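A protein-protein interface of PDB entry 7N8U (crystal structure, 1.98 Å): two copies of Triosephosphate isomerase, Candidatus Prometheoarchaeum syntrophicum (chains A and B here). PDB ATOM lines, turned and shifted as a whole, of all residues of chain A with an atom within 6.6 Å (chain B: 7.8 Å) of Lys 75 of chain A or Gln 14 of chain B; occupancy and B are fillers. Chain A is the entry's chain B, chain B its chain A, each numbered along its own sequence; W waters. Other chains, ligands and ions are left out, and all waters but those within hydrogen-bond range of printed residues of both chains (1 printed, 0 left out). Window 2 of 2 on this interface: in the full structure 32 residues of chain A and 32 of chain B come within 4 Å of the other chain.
Water W1 lies within hydrogen-bond range of the backbone carbonyl oxygen (O) of Asp 85 of chain A (3.0 Å) and the side-chain amide oxygen (OD1) of Asn 17 of chain B (3.1 Å).
No position is printed for both chains.
Of the 17 pairs that touch across the chains among the printed residues, none has its exchanged pair printed and touching as well.
The backbone carbonyl oxygen (O) of Met 13 of chain B is in hydrogen-bond range of the backbone NH (N) of Gly 76 of chain A (3.0 Å).
N of Ser 83 of chain A is in hydrogen-bond range of SD of Met 13 of chain B (3.5 Å).
The backbone NH (N) of Gly 76 of chain A sits at hydrogen-bond distance from the side-chain amide oxygen (OE1) of Gln 14 of chain B, 3.4 Å away.
O of Ala 77 of chain A sits close to OE1 of Glu 101 of chain B, 3.2 Å away.
Of the printed residues of chain B, Asp 74 of chain A touches Met 13 (3.5 Å) and Leu 16 (3.3 Å).
Lys 75 of chain A touches two residues of chain B.
Of chain B, only Lys 12, Met 13 and Gln 14 come within 4 Å of Gly 76 of chain A.
Printed residues of chain B within 4 Å of Asp 85 of chain A: Leu 16 (3.4 Å).
Printed residues of chain A within 4 Å of Lys 12 of chain B: Gly 76, Ala 77 and Phe 78.
Gln 14 of chain B touches just these residues of chain A: Lys 75 (3.4 Å), Gly 76 (3.4 Å) and Ala 77 (3.7 Å).
Hydrophobic or aromatic side chains of chain B that line the printed part of chain A: Met 13 and Leu 16.
Of the 9 printed residues of chain A, 8 touch a printed residue of chain B.
Hydrophobic or aromatic side chains of chain A within 4 Å of the printed part of chain B: Ala 77.
Among the printed residues, 17 pairs touch across the chains.
The backbone NH (N) of Lys 12 of chain B lies within hydrogen-bond range of the side-chain amide oxygen (OD1) of Asn 10 of chain B (3.0 Å).
The side-chain hydroxyl of Ser 47 of chain B is in hydrogen-bond range of the backbone carbonyl oxygen of Lys 12 of chain B (3.0 Å).
The backbone carbonyl oxygen (O) of Lys 12 of chain B lies within hydrogen-bond range of the side-chain amide nitrogen (NE2) of Gln 68 of chain B.
The side-chain carboxylate of Glu 101 of chain B is in salt-bridge range of the side-chain amino group of Lys 12 of chain B (2.8 Å).
The side-chain hydroxyl (OG) of Ser 83 of chain A lies within hydrogen-bond range of the backbone carbonyl oxygen (O) of Asp 74 of chain A (2.7 Å).
N of Asp 85 of chain A lies within hydrogen-bond range of OG of Ser 83 of chain A, 2.9 Å away.
Among the printed residues, merely in contact across the chains: Arg 73 of chain A with Met 13 of chain B, Asp 74 of chain A with Met 13 of chain B, Asp 74 of chain A with Leu 16 of chain B, Lys 75 of chain A with Met 13 of chain B, Lys 75 of chain A with Gln 14 of chain B, Gly 76 of chain A with Lys 12 of chain B, Ala 77 of chain A with Lys 12 of chain B, Ala 77 of chain A with Gln 14 of chain B, Phe 78 of chain A with Lys 12 of chain B, Phe 78 of chain A with Met 13 of chain B, Phe 78 of chain A with Glu 101 of chain B, Ser 83 of chain A with Leu 16 of chain B and Asp 85 of chain A with Leu 16 of chain B.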
ATOM      1  N   ARG A  73     -13.375  19.104  -2.780  1.00  0.00           N
ATOM      2  CA  ARG A  73     -12.229  19.693  -3.452  1.00  0.00           C
ATOM      3  C   ARG A  73     -11.186  18.605  -3.664  1.00  0.00           C
ATOM      4  O   ARG A  73     -11.147  17.619  -2.930  1.00  0.00           O
ATOM      5  CB  ARG A  73     -11.627  20.839  -2.625  1.00  0.00           C
ATOM      6  CG  ARG A  73     -12.542  22.034  -2.424  1.00  0.00           C
ATOM      7  CD  ARG A  73     -12.398  23.067  -3.523  1.00  0.00           C
ATOM      8  NE  ARG A  73     -12.874  24.372  -3.055  1.00  0.00           N
ATOM      9  CZ  ARG A  73     -14.063  24.894  -3.351  1.00  0.00           C
ATOM     10  NH1 ARG A  73     -14.908  24.235  -4.140  1.00  0.00           N
ATOM     11  NH2 ARG A  73     -14.408  26.080  -2.861  1.00  0.00           N
ATOM     12  N   ASP A  74     -10.330  18.795  -4.672  1.00  0.00           N
ATOM     13  CA  ASP A  74      -9.287  17.814  -4.958  1.00  0.00           C
ATOM     14  C   ASP A  74      -8.145  17.874  -3.953  1.00  0.00           C
ATOM     15  O   ASP A  74      -7.526  16.845  -3.658  1.00  0.00           O
ATOM     16  CB  ASP A  74      -8.718  18.044  -6.357  1.00  0.00           C
ATOM     17  CG  ASP A  74      -9.628  17.521  -7.450  1.00  0.00           C
ATOM     18  OD1 ASP A  74      -9.277  17.646  -8.640  1.00  0.00           O
ATOM     19  OD2 ASP A  74     -10.689  16.977  -7.104  1.00  0.00           O
ATOM     20  N   LYS A  75      -7.843  19.065  -3.438  1.00  0.00           N
ATOM     21  CA  LYS A  75      -6.600  19.310  -2.726  1.00  0.00           C
ATOM     22  C   LYS A  75      -6.750  20.616  -1.958  1.00  0.00           C
ATOM     23  O   LYS A  75      -7.468  21.515  -2.398  1.00  0.00           O
ATOM     24  CB  LYS A  75      -5.441  19.364  -3.732  1.00  0.00           C
ATOM     25  CG  LYS A  75      -4.068  19.637  -3.178  1.00  0.00           C
ATOM     26  CD  LYS A  75      -3.109  19.905  -4.334  1.00  0.00           C
ATOM     27  CE  LYS A  75      -1.659  19.837  -3.885  1.00  0.00           C
ATOM     28  NZ  LYS A  75      -0.743  19.976  -5.046  1.00  0.00           N
ATOM     29  N   GLY A  76      -6.100  20.722  -0.807  1.00  0.00           N
ATOM     30  CA  GLY A  76      -6.056  22.002  -0.126  1.00  0.00           C
ATOM     31  C   GLY A  76      -5.954  21.864   1.383  1.00  0.00           C
ATOM     32  O   GLY A  76      -5.635  20.804   1.913  1.00  0.00           O
ATOM     33  N   ALA A  77      -6.230  22.985   2.060  1.00  0.00           N
ATOM     34  CA  ALA A  77      -6.004  23.125   3.503  1.00  0.00           C
ATOM     35  C   ALA A  77      -7.268  22.698   4.243  1.00  0.00           C
ATOM     36  O   ALA A  77      -8.048  23.512   4.748  1.00  0.00           O
ATOM     37  CB  ALA A  77      -5.611  24.559   3.850  1.00  0.00           C
ATOM     38  N   PHE A  78      -7.477  21.383   4.300  1.00  0.00           N
ATOM     39  CA  PHE A  78      -8.681  20.797   4.898  1.00  0.00           C
ATOM     40  C   PHE A  78      -8.244  19.678   5.831  1.00  0.00           C
ATOM     41  O   PHE A  78      -8.293  18.501   5.468  1.00  0.00           O
ATOM     42  CB  PHE A  78      -9.646  20.308   3.795  1.00  0.00           C
ATOM     43  CG  PHE A  78      -9.952  21.358   2.774  1.00  0.00           C
ATOM     44  CD1 PHE A  78      -9.393  21.302   1.493  1.00  0.00           C
ATOM     45  CD2 PHE A  78     -10.775  22.427   3.104  1.00  0.00           C
ATOM     46  CE1 PHE A  78      -9.664  22.301   0.566  1.00  0.00           C
ATOM     47  CE2 PHE A  78     -11.046  23.430   2.175  1.00  0.00           C
ATOM     48  CZ  PHE A  78     -10.490  23.367   0.917  1.00  0.00           C
ATOM     49  N   SER A  83      -9.522  13.385  -0.042  1.00  0.00           N
ATOM     50  CA  SER A  83      -9.761  13.824  -1.412  1.00  0.00           C
ATOM     51  C   SER A  83     -10.358  12.703  -2.261  1.00  0.00           C
ATOM     52  O   SER A  83     -10.025  11.529  -2.067  1.00  0.00           O
ATOM     53  CB  SER A  83      -8.455  14.278  -2.057  1.00  0.00           C
ATOM     54  OG  SER A  83      -8.587  14.384  -3.473  1.00  0.00           O
ATOM     55  N   PRO A  84     -11.210  13.038  -3.244  1.00  0.00           N
ATOM     56  CA  PRO A  84     -11.628  12.012  -4.217  1.00  0.00           C
ATOM     57  C   PRO A  84     -10.445  11.322  -4.863  1.00  0.00           C
ATOM     58  O   PRO A  84     -10.508  10.118  -5.137  1.00  0.00           O
ATOM     59  CB  PRO A  84     -12.446  12.810  -5.249  1.00  0.00           C
ATOM     60  CG  PRO A  84     -12.015  14.251  -5.051  1.00  0.00           C
ATOM     61  CD  PRO A  84     -11.771  14.359  -3.572  1.00  0.00           C
ATOM     62  N   ASP A  85      -9.345  12.048  -5.087  1.00  0.00           N
ATOM     63  CA  ASP A  85      -8.159  11.431  -5.675  1.00  0.00           C
ATOM     64  C   ASP A  85      -7.599  10.338  -4.773  1.00  0.00           C
ATOM     65  O   ASP A  85      -7.073   9.332  -5.267  1.00  0.00           O
ATOM     66  CB  ASP A  85      -7.087  12.493  -5.959  1.00  0.00           C
ATOM     67  CG  ASP A  85      -7.465  13.418  -7.117  1.00  0.00           C
ATOM     68  OD1 ASP A  85      -7.002  14.574  -7.142  1.00  0.00           O
ATOM     69  OD2 ASP A  85      -8.224  13.002  -8.002  1.00  0.00           O
ATOM     70  N   ASN B  10       1.569  19.134   9.548  1.00  0.00           N
ATOM     71  CA  ASN B  10       0.169  18.854   9.212  1.00  0.00           C
ATOM     72  C   ASN B  10       0.037  18.908   7.694  1.00  0.00           C
ATOM     73  O   ASN B  10       0.012  19.988   7.102  1.00  0.00           O
ATOM     74  CB  ASN B  10      -0.749  19.865   9.890  1.00  0.00           C
ATOM     75  CG  ASN B  10      -2.221  19.650   9.565  1.00  0.00           C
ATOM     76  OD1 ASN B  10      -2.620  18.629   8.985  1.00  0.00           O
ATOM     77  ND2 ASN B  10      -3.044  20.619   9.957  1.00  0.00           N
ATOM     78  N   TRP B  11      -0.048  17.738   7.066  1.00  0.00           N
ATOM     79  CA  TRP B  11      -0.147  17.651   5.619  1.00  0.00           C
ATOM     80  C   TRP B  11      -1.544  17.973   5.108  1.00  0.00           C
ATOM     81  O   TRP B  11      -1.730  18.020   3.895  1.00  0.00           O
ATOM     82  CB  TRP B  11       0.268  16.253   5.151  1.00  0.00           C
ATOM     83  CG  TRP B  11       1.751  16.002   5.287  1.00  0.00           C
ATOM     84  CD1 TRP B  11       2.673  16.841   5.841  1.00  0.00           C
ATOM     85  CD2 TRP B  11       2.470  14.834   4.864  1.00  0.00           C
ATOM     86  NE1 TRP B  11       3.929  16.267   5.790  1.00  0.00           N
ATOM     87  CE2 TRP B  11       3.830  15.040   5.182  1.00  0.00           C
ATOM     88  CE3 TRP B  11       2.096  13.637   4.238  1.00  0.00           C
ATOM     89  CZ2 TRP B  11       4.819  14.099   4.895  1.00  0.00           C
ATOM     90  CZ3 TRP B  11       3.087  12.702   3.940  1.00  0.00           C
ATOM     91  CH2 TRP B  11       4.434  12.941   4.271  1.00  0.00           C
ATOM     92  N   LYS B  12      -2.515  18.193   5.997  1.00  0.00           N
ATOM     93  CA  LYS B  12      -3.875  18.568   5.617  1.00  0.00           C
ATOM     94  C   LYS B  12      -4.364  17.697   4.461  1.00  0.00           C
ATOM     95  O   LYS B  12      -4.170  16.478   4.498  1.00  0.00           O
ATOM     96  CB  LYS B  12      -3.933  20.065   5.289  1.00  0.00           C
ATOM     97  CG  LYS B  12      -3.490  20.942   6.483  1.00  0.00           C
ATOM     98  CD  LYS B  12      -3.910  22.398   6.335  1.00  0.00           C
ATOM     99  CE  LYS B  12      -3.419  23.233   7.535  1.00  0.00           C
ATOM    100  NZ  LYS B  12      -3.771  24.683   7.349  1.00  0.00           N
ATOM    101  N   MET B  13      -4.976  18.289   3.427  1.00  0.00           N
ATOM    102  CA  MET B  13      -5.401  17.486   2.280  1.00  0.00           C
ATOM    103  C   MET B  13      -4.599  17.836   1.030  1.00  0.00           C
ATOM    104  O   MET B  13      -5.146  18.018  -0.064  1.00  0.00           O
ATOM    105  CB  MET B  13      -6.936  17.590   2.137  1.00  0.00           C
ATOM    106  CG  MET B  13      -7.608  16.406   1.370  1.00  0.00           C
ATOM    107  SD  MET B  13      -9.332  16.775   0.922  1.00  0.00           S
ATOM    108  CE  MET B  13      -9.116  17.713  -0.596  1.00  0.00           C
ATOM    109  N   GLN B  14      -3.271  17.870   1.198  1.00  0.00           N
ATOM    110  CA  GLN B  14      -2.354  18.311   0.155  1.00  0.00           C
ATOM    111  C   GLN B  14      -1.628  17.171  -0.542  1.00  0.00           C
ATOM    112  O   GLN B  14      -1.149  17.360  -1.662  1.00  0.00           O
ATOM    113  CB  GLN B  14      -1.305  19.276   0.731  1.00  0.00           C
ATOM    114  CG  GLN B  14      -1.876  20.461   1.501  1.00  0.00           C
ATOM    115  CD  GLN B  14      -2.472  21.520   0.601  1.00  0.00           C
ATOM    116  OE1 GLN B  14      -2.735  21.277  -0.577  1.00  0.00           O
ATOM    117  NE2 GLN B  14      -2.698  22.703   1.154  1.00  0.00           N
ATOM    118  N   ILE B  15      -1.530  16.003   0.085  1.00  0.00           N
ATOM    119  CA  ILE B  15      -0.844  14.854  -0.487  1.00  0.00           C
ATOM    120  C   ILE B  15      -1.869  13.748  -0.651  1.00  0.00           C
ATOM    121  O   ILE B  15      -2.411  13.228   0.336  1.00  0.00           O
ATOM    122  CB  ILE B  15       0.349  14.411   0.365  1.00  0.00           C
ATOM    123  CG1 ILE B  15       1.331  15.580   0.470  1.00  0.00           C
ATOM    124  CG2 ILE B  15       0.984  13.136  -0.205  1.00  0.00           C
ATOM    125  CD1 ILE B  15       2.384  15.431   1.543  1.00  0.00           C
ATOM    126  N   LEU B  16      -2.141  13.390  -1.899  1.00  0.00           N
ATOM    127  CA  LEU B  16      -3.343  12.639  -2.211  1.00  0.00           C
ATOM    128  C   LEU B  16      -3.085  11.158  -2.382  1.00  0.00           C
ATOM    129  O   LEU B  16      -3.929  10.351  -1.988  1.00  0.00           O
ATOM    130  CB  LEU B  16      -3.988  13.202  -3.481  1.00  0.00           C
ATOM    131  CG  LEU B  16      -4.157  14.723  -3.410  1.00  0.00           C
ATOM    132  CD1 LEU B  16      -4.797  15.264  -4.685  1.00  0.00           C
ATOM    133  CD2 LEU B  16      -4.936  15.149  -2.160  1.00  0.00           C
ATOM    134  N   ASN B  17      -1.938  10.782  -2.954  1.00  0.00           N
ATOM    135  CA  ASN B  17      -1.639   9.388  -3.260  1.00  0.00           C
ATOM    136  C   ASN B  17      -0.715   8.797  -2.211  1.00  0.00           C
ATOM    137  O   ASN B  17       0.196   9.470  -1.722  1.00  0.00           O
ATOM    138  CB  ASN B  17      -0.981   9.228  -4.633  1.00  0.00           C
ATOM    139  CG  ASN B  17      -1.872   9.673  -5.758  1.00  0.00           C
ATOM    140  OD1 ASN B  17      -3.094   9.677  -5.629  1.00  0.00           O
ATOM    141  ND2 ASN B  17      -1.267  10.030  -6.888  1.00  0.00           N
ATOM    142  N   GLU B  20       3.075   8.859  -2.998  1.00  0.00           N
ATOM    143  CA  GLU B  20       3.743  10.130  -2.735  1.00  0.00           C
ATOM    144  C   GLU B  20       3.919  10.370  -1.243  1.00  0.00           C
ATOM    145  O   GLU B  20       4.969  10.861  -0.809  1.00  0.00           O
ATOM    146  CB  GLU B  20       2.978  11.302  -3.358  1.00  0.00           C
ATOM    147  CG  GLU B  20       3.789  12.595  -3.236  1.00  0.00           C
ATOM    148  CD  GLU B  20       3.087  13.855  -3.721  1.00  0.00           C
ATOM    149  OE1 GLU B  20       1.871  13.827  -3.988  1.00  0.00           O
ATOM    150  OE2 GLU B  20       3.777  14.889  -3.838  1.00  0.00           O
ATOM    151  N   ILE B  24       7.597  11.030   0.369  1.00  0.00           N
ATOM    152  CA  ILE B  24       7.927  12.213   1.162  1.00  0.00           C
ATOM    153  C   ILE B  24       8.325  11.815   2.582  1.00  0.00           C
ATOM    154  O   ILE B  24       9.337  12.285   3.117  1.00  0.00           O
ATOM    155  CB  ILE B  24       6.738  13.190   1.158  1.00  0.00           C
ATOM    156  CG1 ILE B  24       6.502  13.710  -0.268  1.00  0.00           C
ATOM    157  CG2 ILE B  24       6.985  14.333   2.124  1.00  0.00           C
ATOM    158  CD1 ILE B  24       5.224  14.520  -0.438  1.00  0.00           C
ATOM    159  N   SER B  47      -2.774  12.226   5.556  1.00  0.00           N
ATOM    160  CA  SER B  47      -4.200  11.913   5.511  1.00  0.00           C
ATOM    161  C   SER B  47      -4.448  10.441   5.867  1.00  0.00           C
ATOM    162  O   SER B  47      -3.565   9.589   5.751  1.00  0.00           O
ATOM    163  CB  SER B  47      -4.763  12.219   4.120  1.00  0.00           C
ATOM    164  OG  SER B  47      -4.692  13.602   3.842  1.00  0.00           O
ATOM    165  N   GLN B  68      -4.620  13.383  11.650  1.00  0.00           N
ATOM    166  CA  GLN B  68      -5.124  14.756  11.588  1.00  0.00           C
ATOM    167  C   GLN B  68      -6.423  14.954  12.355  1.00  0.00           C
ATOM    168  O   GLN B  68      -6.863  16.099  12.516  1.00  0.00           O
ATOM    169  CB  GLN B  68      -5.352  15.186  10.135  1.00  0.00           C
ATOM    170  CG  GLN B  68      -4.105  15.156   9.270  1.00  0.00           C
ATOM    171  CD  GLN B  68      -4.385  15.594   7.841  1.00  0.00           C
ATOM    172  OE1 GLN B  68      -5.485  16.073   7.517  1.00  0.00           O
ATOM    173  NE2 GLN B  68      -3.403  15.406   6.972  1.00  0.00           N
ATOM    174  N   GLU B 101      -9.536  24.370  11.126  1.00  0.00           N
ATOM    175  CA  GLU B 101     -10.410  23.943  10.037  1.00  0.00           C
ATOM    176  C   GLU B 101     -11.507  23.018  10.554  1.00  0.00           C
ATOM    177  O   GLU B 101     -12.668  23.143  10.146  1.00  0.00           O
ATOM    178  CB  GLU B 101      -9.584  23.301   8.921  1.00  0.00           C
ATOM    179  CG  GLU B 101      -8.776  24.363   8.153  1.00  0.00           C
ATOM    180  CD  GLU B 101      -7.401  23.907   7.740  1.00  0.00           C
ATOM    181  OE1 GLU B 101      -7.144  22.676   7.749  1.00  0.00           O
ATOM    182  OE2 GLU B 101      -6.559  24.796   7.455  1.00  0.00           O
ATOM    183  N   GLY B 245       2.329  23.965   8.335  1.00  0.00           N
ATOM    184  CA  GLY B 245       1.518  23.657   7.176  1.00  0.00           C
ATOM    185  C   GLY B 245       2.334  23.385   5.923  1.00  0.00           C
ATOM    186  O   GLY B 245       2.956  22.324   5.795  1.00  0.00           O
ATOM    187  N   GLY B 246       2.347  24.347   4.993  1.00  0.00           N
ATOM    188  CA  GLY B 246       2.970  24.115   3.695  1.00  0.00           C
ATOM    189  C   GLY B 246       4.436  23.740   3.776  1.00  0.00           C
ATOM    190  O   GLY B 246       4.923  22.951   2.964  1.00  0.00           O
ATOM    191  N   LEU B 249       5.593  19.902   3.793  1.00  0.00           N
ATOM    192  CA  LEU B 249       5.249  19.021   2.687  1.00  0.00           C
ATOM    193  C   LEU B 249       6.464  18.457   1.963  1.00  0.00           C
ATOM    194  O   LEU B 249       6.295  17.638   1.059  1.00  0.00           O
ATOM    195  CB  LEU B 249       4.347  19.759   1.694  1.00  0.00           C
ATOM    196  CG  LEU B 249       2.978  20.160   2.261  1.00  0.00           C
ATOM    197  CD1 LEU B 249       2.179  20.971   1.248  1.00  0.00           C
ATOM    198  CD2 LEU B 249       2.211  18.909   2.699  1.00  0.00           C
HETATM  199  O   HOH W   1      -5.326   9.511  -7.710  1.00  0.00           O
